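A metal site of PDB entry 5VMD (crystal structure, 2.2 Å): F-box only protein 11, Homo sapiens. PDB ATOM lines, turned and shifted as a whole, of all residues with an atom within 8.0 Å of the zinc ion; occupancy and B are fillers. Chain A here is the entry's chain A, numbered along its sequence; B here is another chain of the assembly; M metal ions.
The backbone carbonyl oxygen (O) of Cys 41 is in hydrogen-bond range of the backbone NH (N) of His 46, 3.3 Å away. A ring nitrogen (NE2) of His 46 lies close to the side-chain sulfur (SG) of Cys 63 of chain B, at 3.3 Å. N of Thr 28 lies close to SG of Cys 26, at 3.4 Å. The backbone NH (N) of Cys 26 sits at hydrogen-bond distance from the side-chain amide oxygen (OD1) of Asn 35, at 2.9 Å. The backbone carbonyl oxygen (O) of Cys 29 is in hydrogen-bond range of the side-chain amide nitrogen (ND2) of Asn 35 (3.0 Å).
The zinc ion is bound by a ring nitrogen (ND1) of His 46 (2.0 Å), a ring nitrogen (ND1) of His 49 (2.1 Å), the side-chain sulfur (SG) of Cys 26 (2.3 Å) and the side-chain sulfur (SG) of Cys 29 (2.4 Å).
Four residues have an atom within 4 Å of the zinc ion: Cys 26, Cys 29, His 46 and His 49.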
ATOM      1  N   ARG A  25      -3.491  21.115  16.948  1.00  0.00           N
ATOM      2  CA  ARG A  25      -4.595  21.008  17.886  1.00  0.00           C
ATOM      3  C   ARG A  25      -4.386  22.114  18.908  1.00  0.00           C
ATOM      4  O   ARG A  25      -3.256  22.333  19.362  1.00  0.00           O
ATOM      5  CB  ARG A  25      -4.626  19.636  18.564  1.00  0.00           C
ATOM      6  CG  ARG A  25      -5.749  19.472  19.581  1.00  0.00           C
ATOM      7  CD  ARG A  25      -6.259  18.056  19.594  1.00  0.00           C
ATOM      8  NE  ARG A  25      -6.734  17.698  18.266  1.00  0.00           N
ATOM      9  CZ  ARG A  25      -6.655  16.484  17.738  1.00  0.00           C
ATOM     10  NH1 ARG A  25      -6.113  15.493  18.440  1.00  0.00           N
ATOM     11  NH2 ARG A  25      -7.101  16.262  16.513  1.00  0.00           N
ATOM     12  N   CYS A  26      -5.447  22.827  19.231  1.00  0.00           N
ATOM     13  CA  CYS A  26      -5.370  23.848  20.267  1.00  0.00           C
ATOM     14  C   CYS A  26      -6.116  23.332  21.484  1.00  0.00           C
ATOM     15  O   CYS A  26      -7.338  23.183  21.456  1.00  0.00           O
ATOM     16  CB  CYS A  26      -5.949  25.188  19.814  1.00  0.00           C
ATOM     17  SG  CYS A  26      -5.787  26.403  21.150  1.00  0.00           S
ATOM     18  N   HIS A  27      -5.362  23.027  22.538  1.00  0.00           N
ATOM     19  CA  HIS A  27      -5.967  22.588  23.780  1.00  0.00           C
ATOM     20  C   HIS A  27      -6.556  23.728  24.588  1.00  0.00           C
ATOM     21  O   HIS A  27      -7.340  23.467  25.501  1.00  0.00           O
ATOM     22  CB  HIS A  27      -4.926  21.824  24.601  1.00  0.00           C
ATOM     23  CG  HIS A  27      -4.324  20.665  23.863  1.00  0.00           C
ATOM     24  ND1 HIS A  27      -4.975  19.459  23.727  1.00  0.00           N
ATOM     25  CD2 HIS A  27      -3.144  20.549  23.216  1.00  0.00           C
ATOM     26  CE1 HIS A  27      -4.212  18.639  23.021  1.00  0.00           C
ATOM     27  NE2 HIS A  27      -3.101  19.276  22.699  1.00  0.00           N
ATOM     28  N   THR A  28      -6.224  24.982  24.259  1.00  0.00           N
ATOM     29  CA  THR A  28      -6.903  26.101  24.907  1.00  0.00           C
ATOM     30  C   THR A  28      -8.347  26.217  24.432  1.00  0.00           C
ATOM     31  O   THR A  28      -9.266  26.397  25.239  1.00  0.00           O
ATOM     32  CB  THR A  28      -6.149  27.398  24.654  1.00  0.00           C
ATOM     33  OG1 THR A  28      -4.817  27.281  25.172  1.00  0.00           O
ATOM     34  CG2 THR A  28      -6.854  28.571  25.325  1.00  0.00           C
ATOM     35  N   CYS A  29      -8.554  26.105  23.120  1.00  0.00           N
ATOM     36  CA  CYS A  29      -9.890  26.205  22.528  1.00  0.00           C
ATOM     37  C   CYS A  29     -10.557  24.827  22.496  1.00  0.00           C
ATOM     38  O   CYS A  29     -10.732  24.215  21.445  1.00  0.00           O
ATOM     39  CB  CYS A  29      -9.795  26.830  21.140  1.00  0.00           C
ATOM     40  SG  CYS A  29      -9.156  28.506  21.156  1.00  0.00           S
ATOM     41  N   ASN A  30     -10.932  24.353  23.679  1.00  0.00           N
ATOM     42  CA  ASN A  30     -11.364  22.979  23.846  1.00  0.00           C
ATOM     43  C   ASN A  30     -12.881  22.795  23.812  1.00  0.00           C
ATOM     44  O   ASN A  30     -13.372  21.748  24.225  1.00  0.00           O
ATOM     45  CB  ASN A  30     -10.796  22.405  25.151  1.00  0.00           C
ATOM     46  CG  ASN A  30     -11.329  23.126  26.397  1.00  0.00           C
ATOM     47  OD1 ASN A  30     -12.255  23.925  26.317  1.00  0.00           O
ATOM     48  ND2 ASN A  30     -10.735  22.821  27.546  1.00  0.00           N
ATOM     49  N   ASN A  35      -9.895  19.152  17.876  1.00  0.00           N
ATOM     50  CA  ASN A  35     -10.002  20.081  16.755  1.00  0.00           C
ATOM     51  C   ASN A  35      -8.778  19.951  15.843  1.00  0.00           C
ATOM     52  O   ASN A  35      -7.757  19.357  16.187  1.00  0.00           O
ATOM     53  CB  ASN A  35     -10.160  21.527  17.261  1.00  0.00           C
ATOM     54  CG  ASN A  35      -9.032  21.966  18.190  1.00  0.00           C
ATOM     55  OD1 ASN A  35      -7.852  21.847  17.876  1.00  0.00           O
ATOM     56  ND2 ASN A  35      -9.402  22.466  19.361  1.00  0.00           N
ATOM     57  N   ILE A  37      -6.544  22.603  13.188  1.00  0.00           N
ATOM     58  CA  ILE A  37      -6.308  24.013  12.895  1.00  0.00           C
ATOM     59  C   ILE A  37      -5.120  24.131  11.957  1.00  0.00           C
ATOM     60  O   ILE A  37      -4.106  23.449  12.149  1.00  0.00           O
ATOM     61  CB  ILE A  37      -6.071  24.787  14.199  1.00  0.00           C
ATOM     62  CG1 ILE A  37      -7.290  24.639  15.127  1.00  0.00           C
ATOM     63  CG2 ILE A  37      -5.718  26.259  13.907  1.00  0.00           C
ATOM     64  CD1 ILE A  37      -7.050  25.085  16.551  1.00  0.00           C
ATOM     65  N   CYS A  41      -3.726  29.807  10.977  1.00  0.00           N
ATOM     66  CA  CYS A  41      -4.592  30.122  12.105  1.00  0.00           C
ATOM     67  C   CYS A  41      -3.899  29.915  13.435  1.00  0.00           C
ATOM     68  O   CYS A  41      -4.086  30.704  14.368  1.00  0.00           O
ATOM     69  CB  CYS A  41      -5.893  29.313  12.039  1.00  0.00           C
ATOM     70  SG  CYS A  41      -7.072  29.942  10.834  1.00  0.00           S
ATOM     71  N   ILE A  42      -3.069  28.875  13.550  1.00  0.00           N
ATOM     72  CA  ILE A  42      -2.432  28.639  14.847  1.00  0.00           C
ATOM     73  C   ILE A  42      -1.542  29.813  15.200  1.00  0.00           C
ATOM     74  O   ILE A  42      -1.429  30.178  16.379  1.00  0.00           O
ATOM     75  CB  ILE A  42      -1.664  27.305  14.862  1.00  0.00           C
ATOM     76  CG1 ILE A  42      -1.684  26.717  16.276  1.00  0.00           C
ATOM     77  CG2 ILE A  42      -0.211  27.501  14.394  1.00  0.00           C
ATOM     78  CD1 ILE A  42      -3.106  26.309  16.742  1.00  0.00           C
ATOM     79  N   CYS A  45      -4.385  33.182  15.029  1.00  0.00           N
ATOM     80  CA  CYS A  45      -5.628  33.060  15.784  1.00  0.00           C
ATOM     81  C   CYS A  45      -5.458  32.407  17.143  1.00  0.00           C
ATOM     82  O   CYS A  45      -6.382  32.488  17.957  1.00  0.00           O
ATOM     83  CB  CYS A  45      -6.666  32.283  14.963  1.00  0.00           C
ATOM     84  SG  CYS A  45      -6.941  32.959  13.313  1.00  0.00           S
ATOM     85  N   HIS A  46      -4.315  31.788  17.427  1.00  0.00           N
ATOM     86  CA  HIS A  46      -4.152  31.077  18.700  1.00  0.00           C
ATOM     87  C   HIS A  46      -2.806  31.400  19.323  1.00  0.00           C
ATOM     88  O   HIS A  46      -2.231  30.573  20.042  1.00  0.00           O
ATOM     89  CB  HIS A  46      -4.363  29.569  18.505  1.00  0.00           C
ATOM     90  CG  HIS A  46      -5.695  29.238  17.898  1.00  0.00           C
ATOM     91  ND1 HIS A  46      -6.807  28.930  18.656  1.00  0.00           N
ATOM     92  CD2 HIS A  46      -6.106  29.222  16.606  1.00  0.00           C
ATOM     93  CE1 HIS A  46      -7.840  28.713  17.864  1.00  0.00           C
ATOM     94  NE2 HIS A  46      -7.438  28.895  16.611  1.00  0.00           N
ATOM     95  N   GLN A  47      -2.318  32.619  19.093  1.00  0.00           N
ATOM     96  CA  GLN A  47      -1.060  33.069  19.671  1.00  0.00           C
ATOM     97  C   GLN A  47      -1.090  32.956  21.192  1.00  0.00           C
ATOM     98  O   GLN A  47      -1.987  33.489  21.849  1.00  0.00           O
ATOM     99  CB  GLN A  47      -0.781  34.504  19.256  1.00  0.00           C
ATOM    100  CG  GLN A  47       0.582  35.036  19.669  1.00  0.00           C
ATOM    101  CD  GLN A  47       0.803  36.476  19.244  1.00  0.00           C
ATOM    102  OE1 GLN A  47       0.222  36.947  18.260  1.00  0.00           O
ATOM    103  NE2 GLN A  47       1.652  37.187  19.974  1.00  0.00           N
ATOM    104  N   GLY A  48      -0.090  32.274  21.743  1.00  0.00           N
ATOM    105  CA  GLY A  48       0.012  32.081  23.175  1.00  0.00           C
ATOM    106  C   GLY A  48      -0.819  30.957  23.736  1.00  0.00           C
ATOM    107  O   GLY A  48      -0.761  30.714  24.947  1.00  0.00           O
ATOM    108  N   HIS A  49      -1.580  30.237  22.897  1.00  0.00           N
ATOM    109  CA  HIS A  49      -2.391  29.141  23.377  1.00  0.00           C
ATOM    110  C   HIS A  49      -1.553  27.872  23.508  1.00  0.00           C
ATOM    111  O   HIS A  49      -0.443  27.757  22.995  1.00  0.00           O
ATOM    112  CB  HIS A  49      -3.569  28.899  22.435  1.00  0.00           C
ATOM    113  CG  HIS A  49      -4.579  30.000  22.437  1.00  0.00           C
ATOM    114  ND1 HIS A  49      -5.792  29.897  21.807  1.00  0.00           N
ATOM    115  CD2 HIS A  49      -4.560  31.214  23.023  1.00  0.00           C
ATOM    116  CE1 HIS A  49      -6.478  31.015  21.984  1.00  0.00           C
ATOM    117  NE2 HIS A  49      -5.747  31.826  22.722  1.00  0.00           N
ATOM    118  N   ASP A  50      -2.116  26.898  24.220  1.00  0.00           N
ATOM    119  CA  ASP A  50      -1.457  25.598  24.376  1.00  0.00           C
ATOM    120  C   ASP A  50      -1.769  24.773  23.141  1.00  0.00           C
ATOM    121  O   ASP A  50      -2.814  24.104  23.059  1.00  0.00           O
ATOM    122  CB  ASP A  50      -1.906  24.921  25.662  1.00  0.00           C
ATOM    123  CG  ASP A  50      -1.216  23.588  25.890  1.00  0.00           C
ATOM    124  OD1 ASP A  50      -0.194  23.346  25.222  1.00  0.00           O
ATOM    125  OD2 ASP A  50      -1.682  22.808  26.737  1.00  0.00           O
ATOM    126  N   VAL A  51      -0.873  24.817  22.162  1.00  0.00           N
ATOM    127  CA  VAL A  51      -1.101  24.198  20.873  1.00  0.00           C
ATOM    128  C   VAL A  51      -0.155  23.013  20.709  1.00  0.00           C
ATOM    129  O   VAL A  51       0.892  22.930  21.362  1.00  0.00           O
ATOM    130  CB  VAL A  51      -0.948  25.193  19.709  1.00  0.00           C
ATOM    131  CG1 VAL A  51      -1.844  26.418  19.931  1.00  0.00           C
ATOM    132  CG2 VAL A  51       0.503  25.601  19.533  1.00  0.00           C
ATOM    133  N   CYS B  63     -10.825  26.466  13.087  1.00  0.00           N
ATOM    134  CA  CYS B  63     -10.813  27.912  13.324  1.00  0.00           C
ATOM    135  C   CYS B  63     -11.524  28.636  12.190  1.00  0.00           C
ATOM    136  O   CYS B  63     -12.508  29.353  12.418  1.00  0.00           O
ATOM    137  CB  CYS B  63      -9.372  28.416  13.480  1.00  0.00           C
ATOM    138  SG  CYS B  63      -9.231  30.145  14.090  1.00  0.00           S
ATOM    139  N   LEU B  68     -14.711  27.225  16.840  1.00  0.00           N
ATOM    140  CA  LEU B  68     -14.001  27.523  18.074  1.00  0.00           C
ATOM    141  C   LEU B  68     -14.663  28.718  18.762  1.00  0.00           C
ATOM    142  O   LEU B  68     -15.444  29.457  18.161  1.00  0.00           O
ATOM    143  CB  LEU B  68     -12.524  27.799  17.784  1.00  0.00           C
ATOM    144  CG  LEU B  68     -11.870  26.653  17.005  1.00  0.00           C
ATOM    145  CD1 LEU B  68     -10.405  26.964  16.711  1.00  0.00           C
ATOM    146  CD2 LEU B  68     -11.998  25.328  17.755  1.00  0.00           C
ATOM    147  N   SER B  69     -14.344  28.902  20.045  1.00  0.00           N
ATOM    148  CA  SER B  69     -15.021  29.925  20.837  1.00  0.00           C
ATOM    149  C   SER B  69     -14.843  31.313  20.232  1.00  0.00           C
ATOM    150  O   SER B  69     -15.761  32.139  20.280  1.00  0.00           O
ATOM    151  CB  SER B  69     -14.547  29.905  22.285  1.00  0.00           C
ATOM    152  OG  SER B  69     -13.135  30.022  22.387  1.00  0.00           O
ATOM    153  N   ASN B  70     -13.611  31.612  19.663  1.00  0.00           N
ATOM    154  CA  ASN B  70     -13.405  32.929  19.076  1.00  0.00           C
ATOM    155  C   ASN B  70     -13.470  32.868  17.551  1.00  0.00           C
ATOM    156  O   ASN B  70     -13.033  31.883  16.951  1.00  0.00           O
ATOM    157  CB  ASN B  70     -12.050  33.509  19.495  1.00  0.00           C
ATOM    158  CG  ASN B  70     -11.906  33.632  21.003  1.00  0.00           C
ATOM    159  OD1 ASN B  70     -12.850  33.990  21.701  1.00  0.00           O
ATOM    160  ND2 ASN B  70     -10.721  33.317  21.514  1.00  0.00           N
HETATM  161 ZN    ZN M   1      -6.768  28.389  20.630  1.00  0.00          ZN
